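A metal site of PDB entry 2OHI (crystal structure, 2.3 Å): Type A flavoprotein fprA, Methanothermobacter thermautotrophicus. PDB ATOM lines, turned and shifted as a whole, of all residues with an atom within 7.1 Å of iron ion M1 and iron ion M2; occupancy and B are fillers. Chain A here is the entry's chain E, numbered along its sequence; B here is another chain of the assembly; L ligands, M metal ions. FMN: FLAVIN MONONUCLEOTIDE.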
ATOM      1  N   TYR A  25     -12.165 -17.898   6.795  1.00  0.00           N
ATOM      2  CA  TYR A  25     -10.991 -17.173   6.338  1.00  0.00           C
ATOM      3  C   TYR A  25     -10.326 -16.424   7.507  1.00  0.00           C
ATOM      4  O   TYR A  25     -10.632 -15.265   7.786  1.00  0.00           O
ATOM      5  CB  TYR A  25     -11.328 -16.234   5.171  1.00  0.00           C
ATOM      6  CG  TYR A  25     -10.122 -15.695   4.435  1.00  0.00           C
ATOM      7  CD1 TYR A  25      -8.924 -16.419   4.405  1.00  0.00           C
ATOM      8  CD2 TYR A  25     -10.181 -14.483   3.737  1.00  0.00           C
ATOM      9  CE1 TYR A  25      -7.786 -15.925   3.728  1.00  0.00           C
ATOM     10  CE2 TYR A  25      -9.056 -13.989   3.049  1.00  0.00           C
ATOM     11  CZ  TYR A  25      -7.870 -14.721   3.058  1.00  0.00           C
ATOM     12  OH  TYR A  25      -6.751 -14.255   2.385  1.00  0.00           O
ATOM     13  N   THR A  34     -14.687 -14.697  -3.472  1.00  0.00           N
ATOM     14  CA  THR A  34     -14.044 -14.562  -4.772  1.00  0.00           C
ATOM     15  C   THR A  34     -12.729 -13.780  -4.659  1.00  0.00           C
ATOM     16  O   THR A  34     -12.594 -12.835  -3.859  1.00  0.00           O
ATOM     17  CB  THR A  34     -14.943 -13.860  -5.812  1.00  0.00           C
ATOM     18  OG1 THR A  34     -15.053 -12.451  -5.509  1.00  0.00           O
ATOM     19  CG2 THR A  34     -16.319 -14.474  -5.866  1.00  0.00           C
ATOM     20  N   TYR A  35     -11.760 -14.184  -5.474  1.00  0.00           N
ATOM     21  CA  TYR A  35     -10.557 -13.400  -5.626  1.00  0.00           C
ATOM     22  C   TYR A  35     -10.682 -12.710  -6.961  1.00  0.00           C
ATOM     23  O   TYR A  35     -10.546 -13.328  -8.029  1.00  0.00           O
ATOM     24  CB  TYR A  35      -9.323 -14.296  -5.507  1.00  0.00           C
ATOM     25  CG  TYR A  35      -9.409 -15.262  -4.352  1.00  0.00           C
ATOM     26  CD1 TYR A  35      -9.644 -14.804  -3.059  1.00  0.00           C
ATOM     27  CD2 TYR A  35      -9.275 -16.636  -4.551  1.00  0.00           C
ATOM     28  CE1 TYR A  35      -9.750 -15.685  -1.985  1.00  0.00           C
ATOM     29  CE2 TYR A  35      -9.373 -17.538  -3.486  1.00  0.00           C
ATOM     30  CZ  TYR A  35      -9.610 -17.044  -2.200  1.00  0.00           C
ATOM     31  OH  TYR A  35      -9.704 -17.897  -1.114  1.00  0.00           O
ATOM     32  N   HIS A  83      -2.247  -4.845  -3.651  1.00  0.00           N
ATOM     33  CA  HIS A  83      -2.149  -5.324  -2.278  1.00  0.00           C
ATOM     34  C   HIS A  83      -1.302  -6.585  -2.270  1.00  0.00           C
ATOM     35  O   HIS A  83      -1.379  -7.392  -3.205  1.00  0.00           O
ATOM     36  CB  HIS A  83      -3.560  -5.629  -1.790  1.00  0.00           C
ATOM     37  CG  HIS A  83      -3.670  -5.844  -0.323  1.00  0.00           C
ATOM     38  ND1 HIS A  83      -2.915  -5.160   0.606  1.00  0.00           N
ATOM     39  CD2 HIS A  83      -4.498  -6.652   0.387  1.00  0.00           C
ATOM     40  CE1 HIS A  83      -3.245  -5.558   1.817  1.00  0.00           C
ATOM     41  NE2 HIS A  83      -4.216  -6.455   1.718  1.00  0.00           N
ATOM     42  N   VAL A  84      -0.511  -6.773  -1.206  1.00  0.00           N
ATOM     43  CA  VAL A  84       0.456  -7.876  -1.151  1.00  0.00           C
ATOM     44  C   VAL A  84      -0.064  -9.201  -0.575  1.00  0.00           C
ATOM     45  O   VAL A  84       0.561 -10.242  -0.796  1.00  0.00           O
ATOM     46  CB  VAL A  84       1.775  -7.478  -0.427  1.00  0.00           C
ATOM     47  CG1 VAL A  84       2.257  -6.120  -0.899  1.00  0.00           C
ATOM     48  CG2 VAL A  84       1.620  -7.539   1.081  1.00  0.00           C
ATOM     49  N   GLU A  85      -1.168  -9.172   0.158  1.00  0.00           N
ATOM     50  CA  GLU A  85      -1.680 -10.379   0.828  1.00  0.00           C
ATOM     51  C   GLU A  85      -1.809 -11.568  -0.143  1.00  0.00           C
ATOM     52  O   GLU A  85      -1.946 -11.389  -1.350  1.00  0.00           O
ATOM     53  CB  GLU A  85      -3.002 -10.084   1.571  1.00  0.00           C
ATOM     54  CG  GLU A  85      -3.352 -11.090   2.692  1.00  0.00           C
ATOM     55  CD  GLU A  85      -4.586 -10.682   3.517  1.00  0.00           C
ATOM     56  OE1 GLU A  85      -4.595  -9.552   4.062  1.00  0.00           O
ATOM     57  OE2 GLU A  85      -5.551 -11.491   3.628  1.00  0.00           O
ATOM     58  N   LYS A  86      -1.746 -12.764   0.438  1.00  0.00           N
ATOM     59  CA  LYS A  86      -1.735 -14.055  -0.247  1.00  0.00           C
ATOM     60  C   LYS A  86      -2.842 -14.297  -1.287  1.00  0.00           C
ATOM     61  O   LYS A  86      -2.639 -15.036  -2.249  1.00  0.00           O
ATOM     62  CB  LYS A  86      -1.850 -15.155   0.819  1.00  0.00           C
ATOM     63  CG  LYS A  86      -0.812 -16.248   0.734  1.00  0.00           C
ATOM     64  CD  LYS A  86      -1.133 -17.378   1.702  1.00  0.00           C
ATOM     65  CE  LYS A  86       0.068 -18.310   1.850  1.00  0.00           C
ATOM     66  NZ  LYS A  86      -0.276 -19.592   2.531  1.00  0.00           N
ATOM     67  N   ASP A  87      -4.016 -13.688  -1.075  1.00  0.00           N
ATOM     68  CA  ASP A  87      -5.210 -14.019  -1.878  1.00  0.00           C
ATOM     69  C   ASP A  87      -5.410 -13.106  -3.077  1.00  0.00           C
ATOM     70  O   ASP A  87      -6.469 -13.106  -3.711  1.00  0.00           O
ATOM     71  CB  ASP A  87      -6.477 -14.052  -1.007  1.00  0.00           C
ATOM     72  CG  ASP A  87      -6.729 -12.744  -0.259  1.00  0.00           C
ATOM     73  OD1 ASP A  87      -5.785 -11.926  -0.103  1.00  0.00           O
ATOM     74  OD2 ASP A  87      -7.871 -12.542   0.195  1.00  0.00           O
ATOM     75  N   HIS A  88      -4.382 -12.308  -3.362  1.00  0.00           N
ATOM     76  CA  HIS A  88      -4.386 -11.400  -4.512  1.00  0.00           C
ATOM     77  C   HIS A  88      -3.028 -11.391  -5.165  1.00  0.00           C
ATOM     78  O   HIS A  88      -2.890 -10.877  -6.265  1.00  0.00           O
ATOM     79  CB  HIS A  88      -4.788  -9.977  -4.091  1.00  0.00           C
ATOM     80  CG  HIS A  88      -6.005  -9.944  -3.223  1.00  0.00           C
ATOM     81  ND1 HIS A  88      -7.236 -10.381  -3.656  1.00  0.00           N
ATOM     82  CD2 HIS A  88      -6.167  -9.570  -1.933  1.00  0.00           C
ATOM     83  CE1 HIS A  88      -8.109 -10.267  -2.670  1.00  0.00           C
ATOM     84  NE2 HIS A  88      -7.485  -9.786  -1.610  1.00  0.00           N
ATOM     85  N   HIS A 151      -5.876  -0.712   2.863  1.00  0.00           N
ATOM     86  CA  HIS A 151      -6.049  -1.630   4.002  1.00  0.00           C
ATOM     87  C   HIS A 151      -4.746  -2.003   4.729  1.00  0.00           C
ATOM     88  O   HIS A 151      -4.760  -2.206   5.948  1.00  0.00           O
ATOM     89  CB  HIS A 151      -6.708  -2.877   3.443  1.00  0.00           C
ATOM     90  CG  HIS A 151      -6.596  -2.973   1.957  1.00  0.00           C
ATOM     91  ND1 HIS A 151      -7.512  -2.394   1.101  1.00  0.00           N
ATOM     92  CD2 HIS A 151      -5.638  -3.505   1.172  1.00  0.00           C
ATOM     93  CE1 HIS A 151      -7.129  -2.595  -0.151  1.00  0.00           C
ATOM     94  NE2 HIS A 151      -5.995  -3.265  -0.136  1.00  0.00           N
ATOM     95  N   TRP A 152      -3.645  -2.110   3.973  1.00  0.00           N
ATOM     96  CA  TRP A 152      -2.299  -2.388   4.539  1.00  0.00           C
ATOM     97  C   TRP A 152      -1.315  -1.237   4.224  1.00  0.00           C
ATOM     98  O   TRP A 152      -1.614  -0.373   3.396  1.00  0.00           O
ATOM     99  CB  TRP A 152      -1.755  -3.722   3.984  1.00  0.00           C
ATOM    100  CG  TRP A 152      -2.161  -4.978   4.752  1.00  0.00           C
ATOM    101  CD1 TRP A 152      -3.072  -5.071   5.781  1.00  0.00           C
ATOM    102  CD2 TRP A 152      -1.697  -6.318   4.521  1.00  0.00           C
ATOM    103  NE1 TRP A 152      -3.198  -6.380   6.201  1.00  0.00           N
ATOM    104  CE2 TRP A 152      -2.361  -7.163   5.448  1.00  0.00           C
ATOM    105  CE3 TRP A 152      -0.782  -6.892   3.630  1.00  0.00           C
ATOM    106  CZ2 TRP A 152      -2.128  -8.553   5.502  1.00  0.00           C
ATOM    107  CZ3 TRP A 152      -0.561  -8.276   3.679  1.00  0.00           C
ATOM    108  CH2 TRP A 152      -1.224  -9.085   4.613  1.00  0.00           C
ATOM    109  N   SER A 155      -0.678  -0.850   0.330  1.00  0.00           N
ATOM    110  CA  SER A 155      -1.876  -0.940  -0.513  1.00  0.00           C
ATOM    111  C   SER A 155      -2.132   0.320  -1.346  1.00  0.00           C
ATOM    112  O   SER A 155      -1.699   1.424  -0.983  1.00  0.00           O
ATOM    113  CB  SER A 155      -3.096  -1.241   0.360  1.00  0.00           C
ATOM    114  OG  SER A 155      -2.877  -2.402   1.130  1.00  0.00           O
ATOM    115  N   ASN A 169      -9.122  -2.630  -4.540  1.00  0.00           N
ATOM    116  CA  ASN A 169      -8.674  -3.809  -3.757  1.00  0.00           C
ATOM    117  C   ASN A 169      -9.714  -4.110  -2.679  1.00  0.00           C
ATOM    118  O   ASN A 169     -10.900  -3.975  -2.963  1.00  0.00           O
ATOM    119  CB  ASN A 169      -7.269  -3.627  -3.163  1.00  0.00           C
ATOM    120  CG  ASN A 169      -6.527  -4.955  -3.037  1.00  0.00           C
ATOM    121  OD1 ASN A 169      -5.863  -5.397  -3.979  1.00  0.00           O
ATOM    122  ND2 ASN A 169      -6.641  -5.610  -1.887  1.00  0.00           N
ATOM    123  N   ASP A 170      -9.295  -4.454  -1.466  1.00  0.00           N
ATOM    124  CA  ASP A 170     -10.210  -4.909  -0.390  1.00  0.00           C
ATOM    125  C   ASP A 170     -11.329  -3.941  -0.005  1.00  0.00           C
ATOM    126  O   ASP A 170     -12.423  -4.380   0.335  1.00  0.00           O
ATOM    127  CB  ASP A 170      -9.451  -5.326   0.867  1.00  0.00           C
ATOM    128  CG  ASP A 170      -8.647  -6.606   0.689  1.00  0.00           C
ATOM    129  OD1 ASP A 170      -9.147  -7.559   0.046  1.00  0.00           O
ATOM    130  OD2 ASP A 170      -7.507  -6.653   1.225  1.00  0.00           O
ATOM    131  N   HIS A 175     -17.249 -10.795   1.146  1.00  0.00           N
ATOM    132  CA  HIS A 175     -16.907 -12.195   0.957  1.00  0.00           C
ATOM    133  C   HIS A 175     -18.124 -12.992   0.553  1.00  0.00           C
ATOM    134  O   HIS A 175     -18.803 -13.602   1.391  1.00  0.00           O
ATOM    135  CB  HIS A 175     -16.243 -12.812   2.190  1.00  0.00           C
ATOM    136  CG  HIS A 175     -14.813 -12.397   2.374  1.00  0.00           C
ATOM    137  ND1 HIS A 175     -13.837 -12.651   1.421  1.00  0.00           N
ATOM    138  CD2 HIS A 175     -14.192 -11.752   3.385  1.00  0.00           C
ATOM    139  CE1 HIS A 175     -12.683 -12.165   1.836  1.00  0.00           C
ATOM    140  NE2 HIS A 175     -12.870 -11.621   3.032  1.00  0.00           N
ATOM    141  N   PHE A 198     -18.026  -7.144   6.323  1.00  0.00           N
ATOM    142  CA  PHE A 198     -16.687  -6.861   5.830  1.00  0.00           C
ATOM    143  C   PHE A 198     -16.112  -5.589   6.467  1.00  0.00           C
ATOM    144  O   PHE A 198     -14.984  -5.587   6.955  1.00  0.00           O
ATOM    145  CB  PHE A 198     -16.727  -6.733   4.324  1.00  0.00           C
ATOM    146  CG  PHE A 198     -15.411  -6.937   3.649  1.00  0.00           C
ATOM    147  CD1 PHE A 198     -15.041  -8.190   3.194  1.00  0.00           C
ATOM    148  CD2 PHE A 198     -14.560  -5.859   3.422  1.00  0.00           C
ATOM    149  CE1 PHE A 198     -13.824  -8.374   2.534  1.00  0.00           C
ATOM    150  CE2 PHE A 198     -13.335  -6.036   2.754  1.00  0.00           C
ATOM    151  CZ  PHE A 198     -12.973  -7.311   2.307  1.00  0.00           C
ATOM    152  N   LEU A 202     -12.902  -5.517   9.147  1.00  0.00           N
ATOM    153  CA  LEU A 202     -11.637  -5.113   8.476  1.00  0.00           C
ATOM    154  C   LEU A 202     -11.394  -3.616   8.402  1.00  0.00           C
ATOM    155  O   LEU A 202     -10.239  -3.174   8.373  1.00  0.00           O
ATOM    156  CB  LEU A 202     -11.502  -5.769   7.088  1.00  0.00           C
ATOM    157  CG  LEU A 202     -11.450  -7.311   7.145  1.00  0.00           C
ATOM    158  CD1 LEU A 202     -11.957  -7.972   5.868  1.00  0.00           C
ATOM    159  CD2 LEU A 202     -10.069  -7.848   7.532  1.00  0.00           C
ATOM    160  N   SER A 232     -11.692  -6.381  -4.638  1.00  0.00           N
ATOM    161  CA  SER A 232     -10.968  -7.655  -4.761  1.00  0.00           C
ATOM    162  C   SER A 232     -11.750  -8.857  -4.196  1.00  0.00           C
ATOM    163  O   SER A 232     -11.310 -10.008  -4.296  1.00  0.00           O
ATOM    164  CB  SER A 232      -9.646  -7.547  -4.048  1.00  0.00           C
ATOM    165  OG  SER A 232      -9.875  -7.196  -2.692  1.00  0.00           O
ATOM    166  N   HIS A 233     -12.909  -8.586  -3.592  1.00  0.00           N
ATOM    167  CA  HIS A 233     -13.772  -9.653  -3.102  1.00  0.00           C
ATOM    168  C   HIS A 233     -15.215  -9.373  -3.419  1.00  0.00           C
ATOM    169  O   HIS A 233     -15.708  -8.288  -3.155  1.00  0.00           O
ATOM    170  CB  HIS A 233     -13.606  -9.787  -1.588  1.00  0.00           C
ATOM    171  CG  HIS A 233     -12.271 -10.296  -1.176  1.00  0.00           C
ATOM    172  ND1 HIS A 233     -11.840 -11.566  -1.457  1.00  0.00           N
ATOM    173  CD2 HIS A 233     -11.261  -9.697  -0.487  1.00  0.00           C
ATOM    174  CE1 HIS A 233     -10.624 -11.746  -0.962  1.00  0.00           C
ATOM    175  NE2 HIS A 233     -10.262 -10.632  -0.365  1.00  0.00           N
ATOM    176  N   HIS B 267      -2.080 -17.299   7.682  1.00  0.00           N
ATOM    177  CA  HIS B 267      -1.491 -17.631   6.375  1.00  0.00           C
ATOM    178  C   HIS B 267      -0.382 -18.705   6.470  1.00  0.00           C
ATOM    179  O   HIS B 267       0.098 -19.191   5.440  1.00  0.00           O
ATOM    180  CB  HIS B 267      -0.953 -16.361   5.693  1.00  0.00           C
ATOM    181  CG  HIS B 267      -2.014 -15.381   5.309  1.00  0.00           C
ATOM    182  ND1 HIS B 267      -2.725 -15.480   4.129  1.00  0.00           N
ATOM    183  CD2 HIS B 267      -2.487 -14.273   5.932  1.00  0.00           C
ATOM    184  CE1 HIS B 267      -3.593 -14.487   4.050  1.00  0.00           C
ATOM    185  NE2 HIS B 267      -3.461 -13.738   5.131  1.00  0.00           N
HETATM  186  N1  FMN L   1       0.745  -6.848  10.680  1.00  0.00           N
HETATM  187  C2  FMN L   1       1.257  -5.863  11.517  1.00  0.00           C
HETATM  188  O2  FMN L   1       2.463  -5.770  11.727  1.00  0.00           O
HETATM  189  N3  FMN L   1       0.423  -4.979  12.154  1.00  0.00           N
HETATM  190  C4  FMN L   1      -0.938  -5.053  11.944  1.00  0.00           C
HETATM  191  O4  FMN L   1      -1.642  -4.303  12.601  1.00  0.00           O
HETATM  192  C4A FMN L   1      -1.483  -6.039  11.100  1.00  0.00           C
HETATM  193  N5  FMN L   1      -2.863  -6.128  10.894  1.00  0.00           N
HETATM  194  C5A FMN L   1      -3.367  -7.120  10.048  1.00  0.00           C
HETATM  195  C6  FMN L   1      -4.747  -7.208   9.842  1.00  0.00           C
HETATM  196  C7  FMN L   1      -5.250  -8.207   9.003  1.00  0.00           C
HETATM  197  C7M FMN L   1      -6.712  -8.513   9.045  1.00  0.00           C
HETATM  198  C8  FMN L   1      -4.384  -9.111   8.365  1.00  0.00           C
HETATM  199  C8M FMN L   1      -4.899 -10.231   7.506  1.00  0.00           C
HETATM  200  C9  FMN L   1      -3.009  -9.016   8.594  1.00  0.00           C
HETATM  201  C9A FMN L   1      -2.498  -8.024   9.424  1.00  0.00           C
HETATM  202  N10 FMN L   1      -1.128  -7.935   9.633  1.00  0.00           N
HETATM  203  C10 FMN L   1      -0.627  -6.943  10.465  1.00  0.00           C
HETATM  204  C1' FMN L   1      -0.169  -8.722   8.786  1.00  0.00           C
HETATM  205  C2' FMN L   1       0.020 -10.148   9.314  1.00  0.00           C
HETATM  206  O2' FMN L   1       0.379 -10.135  10.697  1.00  0.00           O
HETATM  207  C3' FMN L   1       1.072 -10.848   8.432  1.00  0.00           C
HETATM  208  O3' FMN L   1       0.595 -11.019   7.103  1.00  0.00           O
HETATM  209  C4' FMN L   1       1.589 -12.177   8.966  1.00  0.00           C
HETATM  210  O4' FMN L   1       2.404 -12.744   7.959  1.00  0.00           O
HETATM  211  C5' FMN L   1       0.518 -13.190   9.360  1.00  0.00           C
HETATM  212  O5' FMN L   1       1.152 -14.286  10.021  1.00  0.00           O
HETATM  213  P   FMN L   1       0.688 -15.797   9.799  1.00  0.00           P
HETATM  214  O1P FMN L   1       1.217 -16.434   8.523  1.00  0.00           O
HETATM  215  O2P FMN L   1       1.116 -16.656  10.967  1.00  0.00           O
HETATM  216  O3P FMN L   1      -0.828 -15.762   9.727  1.00  0.00           O
HETATM  217 FE    FE M   1      -8.345  -9.540   0.426  1.00  0.00          FE
HETATM  218 FE    FE M   2      -5.803  -7.682   2.664  1.00  0.00          FE
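Iron ion M2 is bound by a ring nitrogen (NE2) of His 83 and the side-chain carboxylate (OD2) of Asp 170.
Slightly farther from iron ion M2 lies OE1 of Glu 85 (2.6 Å).
The backbone NH (N) of Asp 170 lies within hydrogen-bond range of the side-chain hydroxyl (OG) of Ser 232, at 3.1 Å.
The side-chain amide nitrogen (ND2) of Asn 169 sits close to the side-chain carboxylate (OD2) of Asp 170.
OG of Ser 155 sits at hydrogen-bond distance from ND1 of His 83 (2.8 Å).
The side-chain carboxylate (OD1) of Asp 87 sits close to a ring nitrogen (NE2) of His 88.
ND1 of His 233 lies within hydrogen-bond range of O of Thr 34, 2.8 Å away.
The side-chain hydroxyl (OH) of Tyr 25 is in hydrogen-bond range of the side-chain carboxylate (OE2) of Glu 85 (3.3 Å).
OE2 of Glu 85 is in hydrogen-bond range of NE2 of His 267 of chain B (3.4 Å).
The side-chain carboxylate (OD2) of Asp 87 is in hydrogen-bond range of the side-chain hydroxyl (OH) of Tyr 25 (3.0 Å).
Within 4 Å of iron ion M2: His 83, Glu 85 and Asp 170.
The nearest printed residue that does not touch iron ion M2 is His 151 (4.4 Å).
An oxygen (O3P) of the ligand lies within hydrogen-bond range of the backbone NH (N) of His 267 of chain B, 2.8 Å away.
Iron ion M1 is bound by the side-chain carboxylate (OD1) of Asp 170, a ring nitrogen (NE2) of His 88 and a ring nitrogen (NE2) of His 233.
Iron ion M1 has three donor atoms within binding distance.
Residues that only touch iron ion M1: Asp 87 (3.0 Å).
Four residues have an atom within 4 Å of iron ion M1: Asp 87, His 88, Asp 170 and His 233.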
